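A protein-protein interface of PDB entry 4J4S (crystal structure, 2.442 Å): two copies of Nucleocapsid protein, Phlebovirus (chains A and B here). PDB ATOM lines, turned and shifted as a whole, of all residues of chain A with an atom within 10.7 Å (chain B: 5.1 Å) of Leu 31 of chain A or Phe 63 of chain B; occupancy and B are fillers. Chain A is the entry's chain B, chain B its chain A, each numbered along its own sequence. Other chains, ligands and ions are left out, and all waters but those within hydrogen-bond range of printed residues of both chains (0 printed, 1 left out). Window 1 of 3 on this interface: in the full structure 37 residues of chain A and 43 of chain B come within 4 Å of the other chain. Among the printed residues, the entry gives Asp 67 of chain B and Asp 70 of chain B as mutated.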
ATOM      1  N   GLU A  23      26.804  -5.484  10.076  1.00  0.00           N
ATOM      2  CA  GLU A  23      26.158  -5.770  11.348  1.00  0.00           C
ATOM      3  C   GLU A  23      24.649  -5.487  11.257  1.00  0.00           C
ATOM      4  O   GLU A  23      23.837  -6.375  11.532  1.00  0.00           O
ATOM      5  CB  GLU A  23      26.821  -4.985  12.485  1.00  0.00           C
ATOM      6  CG  GLU A  23      26.058  -5.072  13.797  1.00  0.00           C
ATOM      7  CD  GLU A  23      26.741  -4.350  14.976  1.00  0.00           C
ATOM      8  OE1 GLU A  23      27.909  -3.909  14.844  1.00  0.00           O
ATOM      9  OE2 GLU A  23      26.102  -4.235  16.047  1.00  0.00           O
ATOM     10  N   LEU A  24      24.272  -4.280  10.818  1.00  0.00           N
ATOM     11  CA  LEU A  24      22.855  -3.896  10.781  1.00  0.00           C
ATOM     12  C   LEU A  24      22.018  -4.713   9.802  1.00  0.00           C
ATOM     13  O   LEU A  24      20.830  -4.952  10.022  1.00  0.00           O
ATOM     14  CB  LEU A  24      22.681  -2.402  10.497  1.00  0.00           C
ATOM     15  CG  LEU A  24      23.462  -1.499  11.451  1.00  0.00           C
ATOM     16  CD1 LEU A  24      23.193  -0.045  11.146  1.00  0.00           C
ATOM     17  CD2 LEU A  24      23.200  -1.828  12.934  1.00  0.00           C
ATOM     18  N   GLU A  25      22.623  -5.158   8.722  1.00  0.00           N
ATOM     19  CA  GLU A  25      21.865  -5.970   7.784  1.00  0.00           C
ATOM     20  C   GLU A  25      21.652  -7.383   8.313  1.00  0.00           C
ATOM     21  O   GLU A  25      20.620  -8.009   8.021  1.00  0.00           O
ATOM     22  CB  GLU A  25      22.520  -5.973   6.395  1.00  0.00           C
ATOM     23  CG  GLU A  25      22.294  -4.660   5.624  1.00  0.00           C
ATOM     24  CD  GLU A  25      23.144  -4.559   4.357  1.00  0.00           C
ATOM     25  OE1 GLU A  25      24.084  -5.364   4.181  1.00  0.00           O
ATOM     26  OE2 GLU A  25      22.876  -3.669   3.539  1.00  0.00           O
ATOM     27  N   ASP A  26      22.625  -7.884   9.087  1.00  0.00           N
ATOM     28  CA  ASP A  26      22.504  -9.195   9.731  1.00  0.00           C
ATOM     29  C   ASP A  26      21.291  -9.128  10.614  1.00  0.00           C
ATOM     30  O   ASP A  26      20.417  -9.994  10.545  1.00  0.00           O
ATOM     31  CB  ASP A  26      23.712  -9.491  10.625  1.00  0.00           C
ATOM     32  CG  ASP A  26      24.951  -9.850   9.835  1.00  0.00           C
ATOM     33  OD1 ASP A  26      24.797 -10.365   8.710  1.00  0.00           O
ATOM     34  OD2 ASP A  26      26.074  -9.613  10.338  1.00  0.00           O
ATOM     35  N   PHE A  27      21.245  -8.080  11.442  1.00  0.00           N
ATOM     36  CA  PHE A  27      20.131  -7.902  12.355  1.00  0.00           C
ATOM     37  C   PHE A  27      18.836  -7.900  11.542  1.00  0.00           C
ATOM     38  O   PHE A  27      17.904  -8.638  11.855  1.00  0.00           O
ATOM     39  CB  PHE A  27      20.287  -6.612  13.182  1.00  0.00           C
ATOM     40  CG  PHE A  27      21.512  -6.601  14.094  1.00  0.00           C
ATOM     41  CD1 PHE A  27      22.225  -7.773  14.366  1.00  0.00           C
ATOM     42  CD2 PHE A  27      21.943  -5.414  14.681  1.00  0.00           C
ATOM     43  CE1 PHE A  27      23.339  -7.752  15.222  1.00  0.00           C
ATOM     44  CE2 PHE A  27      23.048  -5.392  15.518  1.00  0.00           C
ATOM     45  CZ  PHE A  27      23.746  -6.567  15.797  1.00  0.00           C
ATOM     46  N   ALA A  28      18.804  -7.120  10.463  1.00  0.00           N
ATOM     47  CA  ALA A  28      17.593  -6.978   9.672  1.00  0.00           C
ATOM     48  C   ALA A  28      17.126  -8.321   9.148  1.00  0.00           C
ATOM     49  O   ALA A  28      15.978  -8.716   9.366  1.00  0.00           O
ATOM     50  CB  ALA A  28      17.801  -5.990   8.522  1.00  0.00           C
ATOM     51  N   ARG A  29      18.018  -9.029   8.468  1.00  0.00           N
ATOM     52  CA  ARG A  29      17.663 -10.338   7.920  1.00  0.00           C
ATOM     53  C   ARG A  29      17.211 -11.318   9.000  1.00  0.00           C
ATOM     54  O   ARG A  29      16.239 -12.049   8.808  1.00  0.00           O
ATOM     55  CB  ARG A  29      18.820 -10.942   7.120  1.00  0.00           C
ATOM     56  CG  ARG A  29      19.350 -10.031   6.054  1.00  0.00           C
ATOM     57  CD  ARG A  29      19.464 -10.734   4.759  1.00  0.00           C
ATOM     58  NE  ARG A  29      19.846  -9.827   3.695  1.00  0.00           N
ATOM     59  CZ  ARG A  29      19.271  -9.822   2.497  1.00  0.00           C
ATOM     60  NH1 ARG A  29      18.304 -10.685   2.210  1.00  0.00           N
ATOM     61  NH2 ARG A  29      19.680  -8.960   1.585  1.00  0.00           N
ATOM     62  N   GLU A  30      17.896 -11.344  10.133  1.00  0.00           N
ATOM     63  CA  GLU A  30      17.527 -12.342  11.135  1.00  0.00           C
ATOM     64  C   GLU A  30      16.224 -11.993  11.870  1.00  0.00           C
ATOM     65  O   GLU A  30      15.568 -12.873  12.422  1.00  0.00           O
ATOM     66  CB  GLU A  30      18.683 -12.660  12.101  1.00  0.00           C
ATOM     67  CG  GLU A  30      18.986 -11.597  13.136  1.00  0.00           C
ATOM     68  CD  GLU A  30      20.200 -11.949  13.996  1.00  0.00           C
ATOM     69  OE1 GLU A  30      21.211 -11.212  13.933  1.00  0.00           O
ATOM     70  OE2 GLU A  30      20.142 -12.951  14.746  1.00  0.00           O
ATOM     71  N   LEU A  31      15.827 -10.720  11.836  1.00  0.00           N
ATOM     72  CA  LEU A  31      14.600 -10.296  12.515  1.00  0.00           C
ATOM     73  C   LEU A  31      13.395 -10.190  11.576  1.00  0.00           C
ATOM     74  O   LEU A  31      12.268  -9.988  12.026  1.00  0.00           O
ATOM     75  CB  LEU A  31      14.826  -8.971  13.250  1.00  0.00           C
ATOM     76  CG  LEU A  31      15.754  -9.037  14.467  1.00  0.00           C
ATOM     77  CD1 LEU A  31      16.153  -7.652  14.956  1.00  0.00           C
ATOM     78  CD2 LEU A  31      15.064  -9.803  15.574  1.00  0.00           C
ATOM     79  N   ALA A  32      13.638 -10.324  10.277  1.00  0.00           N
ATOM     80  CA  ALA A  32      12.584 -10.162   9.287  1.00  0.00           C
ATOM     81  C   ALA A  32      11.411 -11.122   9.460  1.00  0.00           C
ATOM     82  O   ALA A  32      11.567 -12.347   9.433  1.00  0.00           O
ATOM     83  CB  ALA A  32      13.151 -10.259   7.899  1.00  0.00           C
ATOM     84  N   TYR A  33      10.236 -10.526   9.642  1.00  0.00           N
ATOM     85  CA  TYR A  33       8.977 -11.224   9.874  1.00  0.00           C
ATOM     86  C   TYR A  33       8.373 -11.729   8.562  1.00  0.00           C
ATOM     87  O   TYR A  33       8.176 -10.976   7.623  1.00  0.00           O
ATOM     88  CB  TYR A  33       8.020 -10.263  10.589  1.00  0.00           C
ATOM     89  CG  TYR A  33       6.613 -10.770  10.825  1.00  0.00           C
ATOM     90  CD1 TYR A  33       6.284 -11.470  11.981  1.00  0.00           C
ATOM     91  CD2 TYR A  33       5.605 -10.513   9.908  1.00  0.00           C
ATOM     92  CE1 TYR A  33       4.986 -11.915  12.205  1.00  0.00           C
ATOM     93  CE2 TYR A  33       4.313 -10.949  10.119  1.00  0.00           C
ATOM     94  CZ  TYR A  33       4.007 -11.658  11.261  1.00  0.00           C
ATOM     95  OH  TYR A  33       2.713 -12.093  11.455  1.00  0.00           O
ATOM     96  N   GLU A  34       8.064 -13.010   8.510  1.00  0.00           N
ATOM     97  CA  GLU A  34       7.667 -13.640   7.261  1.00  0.00           C
ATOM     98  C   GLU A  34       6.192 -13.420   6.944  1.00  0.00           C
ATOM     99  O   GLU A  34       5.797 -13.360   5.774  1.00  0.00           O
ATOM    100  CB  GLU A  34       7.968 -15.138   7.332  1.00  0.00           C
ATOM    101  CG  GLU A  34       7.962 -15.835   5.995  1.00  0.00           C
ATOM    102  CD  GLU A  34       8.399 -17.294   6.075  1.00  0.00           C
ATOM    103  OE1 GLU A  34       7.962 -18.071   5.198  1.00  0.00           O
ATOM    104  OE2 GLU A  34       9.178 -17.658   6.995  1.00  0.00           O
ATOM    105  N   GLY A  35       5.381 -13.297   7.990  1.00  0.00           N
ATOM    106  CA  GLY A  35       3.939 -13.264   7.843  1.00  0.00           C
ATOM    107  C   GLY A  35       3.375 -14.579   7.343  1.00  0.00           C
ATOM    108  O   GLY A  35       3.286 -15.567   8.076  1.00  0.00           O
ATOM    109  N   ARG A 102       2.865 -19.097  13.027  1.00  0.00           N
ATOM    110  CA  ARG A 102       3.164 -19.189  11.595  1.00  0.00           C
ATOM    111  C   ARG A 102       2.524 -20.429  10.951  1.00  0.00           C
ATOM    112  O   ARG A 102       2.382 -20.501   9.730  1.00  0.00           O
ATOM    113  CB  ARG A 102       4.678 -19.195  11.350  1.00  0.00           C
ATOM    114  CG  ARG A 102       5.417 -20.332  12.051  1.00  0.00           C
ATOM    115  CD  ARG A 102       6.645 -20.815  11.263  1.00  0.00           C
ATOM    116  NE  ARG A 102       7.732 -19.833  11.250  1.00  0.00           N
ATOM    117  CZ  ARG A 102       8.160 -19.207  10.156  1.00  0.00           C
ATOM    118  NH1 ARG A 102       7.595 -19.464   8.986  1.00  0.00           N
ATOM    119  NH2 ARG A 102       9.154 -18.324  10.229  1.00  0.00           N
ATOM    120  N   ALA A 206       5.084  -6.057   2.639  1.00  0.00           N
ATOM    121  CA  ALA A 206       5.755  -7.294   3.042  1.00  0.00           C
ATOM    122  C   ALA A 206       7.270  -7.170   3.174  1.00  0.00           C
ATOM    123  O   ALA A 206       7.887  -6.213   2.697  1.00  0.00           O
ATOM    124  CB  ALA A 206       5.410  -8.424   2.072  1.00  0.00           C
ATOM    125  N   ALA A 207       7.851  -8.173   3.822  1.00  0.00           N
ATOM    126  CA  ALA A 207       9.270  -8.196   4.155  1.00  0.00           C
ATOM    127  C   ALA A 207      10.102  -8.889   3.076  1.00  0.00           C
ATOM    128  O   ALA A 207       9.563  -9.511   2.153  1.00  0.00           O
ATOM    129  CB  ALA A 207       9.466  -8.881   5.482  1.00  0.00           C
ATOM    130  N   VAL A 208      11.422  -8.779   3.203  1.00  0.00           N
ATOM    131  CA  VAL A 208      12.348  -9.415   2.263  1.00  0.00           C
ATOM    132  C   VAL A 208      12.202 -10.937   2.363  1.00  0.00           C
ATOM    133  O   VAL A 208      12.431 -11.683   1.406  1.00  0.00           O
ATOM    134  CB  VAL A 208      13.797  -8.927   2.532  1.00  0.00           C
ATOM    135  CG1 VAL A 208      14.838  -9.899   1.994  1.00  0.00           C
ATOM    136  CG2 VAL A 208      13.994  -7.502   1.962  1.00  0.00           C
ATOM    137  N   ASN A 209      11.753 -11.367   3.533  1.00  0.00           N
ATOM    138  CA  ASN A 209      11.540 -12.771   3.863  1.00  0.00           C
ATOM    139  C   ASN A 209      10.332 -13.421   3.165  1.00  0.00           C
ATOM    140  O   ASN A 209      10.247 -14.651   3.055  1.00  0.00           O
ATOM    141  CB  ASN A 209      11.387 -12.882   5.394  1.00  0.00           C
ATOM    142  CG  ASN A 209      11.327 -14.313   5.874  1.00  0.00           C
ATOM    143  OD1 ASN A 209      10.921 -14.584   7.009  1.00  0.00           O
ATOM    144  ND2 ASN A 209      11.726 -15.248   5.009  1.00  0.00           N
ATOM    145  N   SER A 210       9.398 -12.597   2.705  1.00  0.00           N
ATOM    146  CA  SER A 210       8.096 -13.091   2.281  1.00  0.00           C
ATOM    147  C   SER A 210       8.130 -13.698   0.892  1.00  0.00           C
ATOM    148  O   SER A 210       9.082 -13.495   0.129  1.00  0.00           O
ATOM    149  CB  SER A 210       7.084 -11.956   2.315  1.00  0.00           C
ATOM    150  OG  SER A 210       7.550 -10.888   1.509  1.00  0.00           O
ATOM    151  N   PHE B  59      20.425  -3.581  18.225  1.00  0.00           N
ATOM    152  CA  PHE B  59      19.689  -4.769  17.790  1.00  0.00           C
ATOM    153  C   PHE B  59      18.199  -4.551  18.059  1.00  0.00           C
ATOM    154  O   PHE B  59      17.349  -5.028  17.321  1.00  0.00           O
ATOM    155  CB  PHE B  59      20.184  -6.037  18.536  1.00  0.00           C
ATOM    156  CG  PHE B  59      19.505  -7.308  18.087  1.00  0.00           C
ATOM    157  CD1 PHE B  59      18.295  -7.698  18.646  1.00  0.00           C
ATOM    158  CD2 PHE B  59      20.072  -8.101  17.094  1.00  0.00           C
ATOM    159  CE1 PHE B  59      17.651  -8.841  18.218  1.00  0.00           C
ATOM    160  CE2 PHE B  59      19.441  -9.252  16.661  1.00  0.00           C
ATOM    161  CZ  PHE B  59      18.226  -9.626  17.228  1.00  0.00           C
ATOM    162  N   ILE B  60      17.887  -3.854  19.142  1.00  0.00           N
ATOM    163  CA  ILE B  60      16.502  -3.609  19.523  1.00  0.00           C
ATOM    164  C   ILE B  60      15.881  -2.538  18.604  1.00  0.00           C
ATOM    165  O   ILE B  60      14.706  -2.609  18.217  1.00  0.00           O
ATOM    166  CB  ILE B  60      16.432  -3.184  21.027  1.00  0.00           C
ATOM    167  CG1 ILE B  60      16.725  -4.405  21.937  1.00  0.00           C
ATOM    168  CG2 ILE B  60      15.091  -2.516  21.370  1.00  0.00           C
ATOM    169  CD1 ILE B  60      17.052  -4.035  23.411  1.00  0.00           C
ATOM    170  N   ILE B  61      16.705  -1.560  18.250  1.00  0.00           N
ATOM    171  CA  ILE B  61      16.289  -0.474  17.398  1.00  0.00           C
ATOM    172  C   ILE B  61      15.924  -0.998  16.006  1.00  0.00           C
ATOM    173  O   ILE B  61      14.934  -0.556  15.428  1.00  0.00           O
ATOM    174  CB  ILE B  61      17.361   0.612  17.347  1.00  0.00           C
ATOM    175  CG1 ILE B  61      17.429   1.328  18.716  1.00  0.00           C
ATOM    176  CG2 ILE B  61      17.056   1.596  16.222  1.00  0.00           C
ATOM    177  CD1 ILE B  61      18.383   2.532  18.759  1.00  0.00           C
ATOM    178  N   VAL B  62      16.705  -1.966  15.504  1.00  0.00           N
ATOM    179  CA  VAL B  62      16.436  -2.604  14.216  1.00  0.00           C
ATOM    180  C   VAL B  62      15.185  -3.480  14.304  1.00  0.00           C
ATOM    181  O   VAL B  62      14.462  -3.645  13.313  1.00  0.00           O
ATOM    182  CB  VAL B  62      17.639  -3.472  13.719  1.00  0.00           C
ATOM    183  CG1 VAL B  62      17.308  -4.146  12.401  1.00  0.00           C
ATOM    184  CG2 VAL B  62      18.904  -2.630  13.577  1.00  0.00           C
ATOM    185  N   PHE B  63      14.942  -4.072  15.478  1.00  0.00           N
ATOM    186  CA  PHE B  63      13.660  -4.727  15.695  1.00  0.00           C
ATOM    187  C   PHE B  63      12.547  -3.673  15.666  1.00  0.00           C
ATOM    188  O   PHE B  63      11.446  -3.944  15.189  1.00  0.00           O
ATOM    189  CB  PHE B  63      13.580  -5.510  17.004  1.00  0.00           C
ATOM    190  CG  PHE B  63      12.226  -6.115  17.237  1.00  0.00           C
ATOM    191  CD1 PHE B  63      11.860  -7.273  16.582  1.00  0.00           C
ATOM    192  CD2 PHE B  63      11.302  -5.491  18.067  1.00  0.00           C
ATOM    193  CE1 PHE B  63      10.616  -7.833  16.778  1.00  0.00           C
ATOM    194  CE2 PHE B  63      10.046  -6.027  18.248  1.00  0.00           C
ATOM    195  CZ  PHE B  63       9.702  -7.203  17.605  1.00  0.00           C
ATOM    196  N   ALA B  64      12.838  -2.477  16.178  1.00  0.00           N
ATOM    197  CA  ALA B  64      11.843  -1.410  16.238  1.00  0.00           C
ATOM    198  C   ALA B  64      11.482  -0.987  14.831  1.00  0.00           C
ATOM    199  O   ALA B  64      10.308  -0.961  14.477  1.00  0.00           O
ATOM    200  CB  ALA B  64      12.372  -0.242  16.996  1.00  0.00           C
ATOM    201  N   LEU B  65      12.514  -0.683  14.042  1.00  0.00           N
ATOM    202  CA  LEU B  65      12.399  -0.218  12.654  1.00  0.00           C
ATOM    203  C   LEU B  65      11.637  -1.160  11.727  1.00  0.00           C
ATOM    204  O   LEU B  65      10.873  -0.719  10.874  1.00  0.00           O
ATOM    205  CB  LEU B  65      13.797  -0.017  12.072  1.00  0.00           C
ATOM    206  CG  LEU B  65      14.556   1.187  12.613  1.00  0.00           C
ATOM    207  CD1 LEU B  65      15.993   1.081  12.161  1.00  0.00           C
ATOM    208  CD2 LEU B  65      13.923   2.433  12.034  1.00  0.00           C
ATOM    209  N   THR B  66      11.848  -2.455  11.917  1.00  0.00           N
ATOM    210  CA  THR B  66      11.352  -3.475  10.998  1.00  0.00           C
ATOM    211  C   THR B  66      10.083  -4.192  11.498  1.00  0.00           C
ATOM    212  O   THR B  66       9.278  -4.654  10.704  1.00  0.00           O
ATOM    213  CB  THR B  66      12.457  -4.525  10.690  1.00  0.00           C
ATOM    214  OG1 THR B  66      12.780  -5.275  11.879  1.00  0.00           O
ATOM    215  CG2 THR B  66      13.724  -3.847  10.152  1.00  0.00           C
ATOM    216  N   ASP B  67       9.899  -4.300  12.808  1.00  0.00           N
ATOM    217  CA  ASP B  67       8.779  -5.097  13.320  1.00  0.00           C
ATOM    218  C   ASP B  67       7.863  -4.360  14.293  1.00  0.00           C
ATOM    219  O   ASP B  67       6.796  -4.870  14.653  1.00  0.00           O
ATOM    220  CB  ASP B  67       9.297  -6.378  13.985  1.00  0.00           C
ATOM    221  CG  ASP B  67      10.028  -7.265  13.015  1.00  0.00           C
ATOM    222  OD1 ASP B  67       9.520  -7.443  11.881  1.00  0.00           O
ATOM    223  OD2 ASP B  67      11.113  -7.774  13.373  1.00  0.00           O
ATOM    224  N   GLY B  68       8.289  -3.177  14.720  1.00  0.00           N
ATOM    225  CA  GLY B  68       7.540  -2.410  15.701  1.00  0.00           C
ATOM    226  C   GLY B  68       7.778  -2.892  17.119  1.00  0.00           C
ATOM    227  O   GLY B  68       8.916  -3.114  17.513  1.00  0.00           O
ATOM    228  N   ASN B  69       6.696  -3.050  17.875  1.00  0.00           N
ATOM    229  CA  ASN B  69       6.742  -3.438  19.279  1.00  0.00           C
ATOM    230  C   ASN B  69       6.252  -4.869  19.463  1.00  0.00           C
ATOM    231  O   ASN B  69       6.125  -5.337  20.598  1.00  0.00           O
ATOM    232  CB  ASN B  69       5.827  -2.519  20.092  1.00  0.00           C
ATOM    233  CG  ASN B  69       6.494  -1.218  20.495  1.00  0.00           C
ATOM    234  OD1 ASN B  69       7.718  -1.133  20.596  1.00  0.00           O
ATOM    235  ND2 ASN B  69       5.680  -0.193  20.751  1.00  0.00           N
ATOM    236  N   ASP B  70       5.971  -5.546  18.345  1.00  0.00           N
ATOM    237  CA  ASP B  70       5.304  -6.850  18.347  1.00  0.00           C
ATOM    238  C   ASP B  70       6.249  -8.005  18.608  1.00  0.00           C
ATOM    239  O   ASP B  70       6.414  -8.893  17.752  1.00  0.00           O
ATOM    240  CB  ASP B  70       4.650  -7.112  16.998  1.00  0.00           C
ATOM    241  CG  ASP B  70       3.596  -6.109  16.661  1.00  0.00           C
ATOM    242  OD1 ASP B  70       3.021  -5.520  17.606  1.00  0.00           O
ATOM    243  OD2 ASP B  70       3.350  -5.908  15.447  1.00  0.00           O
ATOM    244  N   ILE B  71       6.847  -8.009  19.792  1.00  0.00           N
ATOM    245  CA  ILE B  71       7.876  -8.980  20.133  1.00  0.00           C
ATOM    246  C   ILE B  71       7.441 -10.431  19.955  1.00  0.00           C
ATOM    247  O   ILE B  71       8.094 -11.198  19.249  1.00  0.00           O
ATOM    248  CB  ILE B  71       8.378  -8.754  21.538  1.00  0.00           C
ATOM    249  CG1 ILE B  71       9.102  -7.415  21.597  1.00  0.00           C
ATOM    250  CG2 ILE B  71       9.278  -9.917  21.950  1.00  0.00           C
ATOM    251  CD1 ILE B  71       9.280  -6.873  22.975  1.00  0.00           C
ATOM    252  N   ALA B  74       6.123 -11.404  16.235  1.00  0.00           N
ATOM    253  CA  ALA B  74       7.304 -11.430  15.369  1.00  0.00           C
ATOM    254  C   ALA B  74       8.241 -12.629  15.610  1.00  0.00           C
ATOM    255  O   ALA B  74       8.749 -13.236  14.649  1.00  0.00           O
ATOM    256  CB  ALA B  74       8.074 -10.113  15.460  1.00  0.00           C
ATOM    257  N   MET B  78      10.011 -15.310  12.624  1.00  0.00           N
ATOM    258  CA  MET B  78      11.339 -14.919  12.186  1.00  0.00           C
ATOM    259  C   MET B  78      12.335 -16.072  12.178  1.00  0.00           C
ATOM    260  O   MET B  78      11.956 -17.239  12.361  1.00  0.00           O
ATOM    261  CB  MET B  78      11.848 -13.741  13.002  1.00  0.00           C
ATOM    262  CG  MET B  78      12.138 -14.064  14.424  1.00  0.00           C
ATOM    263  SD  MET B  78      12.859 -12.628  15.190  1.00  0.00           S
ATOM    264  CE  MET B  78      11.421 -11.568  15.330  1.00  0.00           C
ATOM    265  N   SER B  79      13.608 -15.763  11.947  1.00  0.00           N
ATOM    266  CA  SER B  79      14.625 -16.819  11.935  1.00  0.00           C
ATOM    267  C   SER B  79      14.842 -17.295  13.366  1.00  0.00           C
ATOM    268  O   SER B  79      14.598 -16.551  14.322  1.00  0.00           O
ATOM    269  CB  SER B  79      15.947 -16.292  11.403  1.00  0.00           C
ATOM    270  OG  SER B  79      16.486 -15.349  12.328  1.00  0.00           O
ATOM    271  N   GLY B  82      17.339 -15.194  15.152  1.00  0.00           N
ATOM    272  CA  GLY B  82      16.768 -13.890  15.489  1.00  0.00           C
ATOM    273  C   GLY B  82      15.811 -13.928  16.674  1.00  0.00           C
ATOM    274  O   GLY B  82      15.916 -13.126  17.605  1.00  0.00           O
ATOM    275  N   LEU B  86      16.251 -12.092  20.293  1.00  0.00           N
ATOM    276  CA  LEU B  86      15.128 -11.266  20.695  1.00  0.00           C
ATOM    277  C   LEU B  86      14.487 -11.744  21.999  1.00  0.00           C
ATOM    278  O   LEU B  86      14.287 -10.946  22.902  1.00  0.00           O
ATOM    279  CB  LEU B  86      14.095 -11.195  19.578  1.00  0.00           C
ATOM    280  CG  LEU B  86      12.886 -10.294  19.804  1.00  0.00           C
ATOM    281  CD1 LEU B  86      13.282  -8.837  19.868  1.00  0.00           C
ATOM    282  CD2 LEU B  86      11.903 -10.525  18.673  1.00  0.00           C
ATOM    283  N   PRO B 107      10.570  -1.474  22.425  1.00  0.00           N
ATOM    284  CA  PRO B 107      11.562  -1.280  21.376  1.00  0.00           C
ATOM    285  C   PRO B 107      11.341   0.024  20.601  1.00  0.00           C
ATOM    286  O   PRO B 107      12.261   0.696  20.251  1.00  0.00           O
ATOM    287  CB  PRO B 107      11.423  -2.511  20.508  1.00  0.00           C
ATOM    288  CG  PRO B 107      10.299  -3.291  21.047  1.00  0.00           C
ATOM    289  CD  PRO B 107       9.943  -2.789  22.374  1.00  0.00           C
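The side-chain hydroxyl of Ser 79 of chain B lies within hydrogen-bond range of the backbone carbonyl oxygen of Glu 30 of chain A, 2.6 Å away. O of Leu 31 of chain A lies close to OD2 of Asp 67 of chain B.
The backbone carbonyl oxygen (O) of Val 62 of chain B lies within hydrogen-bond range of the side-chain hydroxyl (OG1) of Thr 66 of chain B. The backbone NH (N) of Gly 68 of chain B lies within hydrogen-bond range of the backbone carbonyl oxygen (O) of Phe 63 of chain B, 3.3 Å away. OG1 of Thr 66 of chain B sits at hydrogen-bond distance from OD2 of Asp 67 of chain B, 3.4 Å away. OG of Ser 79 of chain B is in hydrogen-bond range of N of Gly 82 of chain B (3.0 Å). The side-chain amide oxygen (OD1) of Asn 209 of chain A sits close to the backbone carbonyl oxygen (O) of Ala 32 of chain A (3.4 Å). OE2 of Glu 34 of chain A is in salt-bridge range of NH1 of Arg 102 of chain A (3.1 Å).
Among the printed residues, pairs that only touch across the chains: Tyr 33 of chain A with Asp 67 of chain B, Glu 30 of chain A with Gly 82 of chain B, Phe 27 of chain A with Phe 59 of chain B, Tyr 33 of chain A with Ala 74 of chain B, Leu 31 of chain A with Phe 59 of chain B, Leu 31 of chain A with Met 78 of chain B, Arg 102 of chain A with Met 78 of chain B, Ala 32 of chain A with Met 78 of chain B, Glu 30 of chain A with Phe 59 of chain B, Leu 31 of chain A with Phe 63 of chain B, Ala 28 of chain A with Val 62 of chain B, Glu 30 of chain A with Met 78 of chain B, Phe 27 of chain A with Val 62 of chain B and Leu 31 of chain A with Gly 82 of chain B.
Glu 25 of chain A touches none of the printed residues of chain B. Of the printed residues of chain B, Ala 28 of chain A touches Val 62. Of the printed residues of chain B, Glu 30 of chain A touches Phe 59, Met 78, Ser 79 and Gly 82. Of the printed residues of chain B, Leu 31 of chain A touches Phe 59 (3.6 Å), Phe 63 (3.8 Å), Asp 67 (2.8 Å), Met 78 (3.6 Å) and Gly 82 (3.99 Å). Ser 210 of chain A touches none of the printed residues of chain B. Phe 59 of chain B touches three residues of chain A. Phe 63 of chain B touches one residue of chain A. No residue of chain A comes within 4 Å of Ala 64 of chain B. No residue of chain A comes within 4 Å of Thr 66 of chain B. Asp 67 of chain B touches just these residues of chain A: Leu 31 (2.8 Å) and Tyr 33 (3.4 Å). No residue of chain A comes within 4 Å of Gly 68 of chain B. No residue of chain A comes within 4 Å of Ile 71 of chain B. Of chain A, only Tyr 33 (3.5 Å) comes within 4 Å of Ala 74 of chain B. Of the printed residues of chain A, Met 78 of chain B touches Glu 30 (3.9 Å), Leu 31 (3.6 Å), Ala 32 (3.8 Å) and Arg 102 (3.7 Å). Of the printed residues of chain A, Ser 79 of chain B touches Glu 30. Printed residues of chain A within 4 Å of Gly 82 of chain B: Glu 30 (3.4 Å) and Leu 31 (3.99 Å). No residue of chain A comes within 4 Å of Pro 107 of chain B.
Hydrophobic or aromatic side chains of chain B that line the printed part of chain A: Phe 59, Val 62, Phe 63 and Met 78. Among the printed residues, 16 pairs touch across the chains. Among the printed residues, no Asp or Glu carboxylate lies within 4 Å of a Lys or Arg side-chain nitrogen of the other chain.
No position is printed for both chains. Of the 16 pairs that touch across the chains among the printed residues, none has its exchanged pair printed and touching as well.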
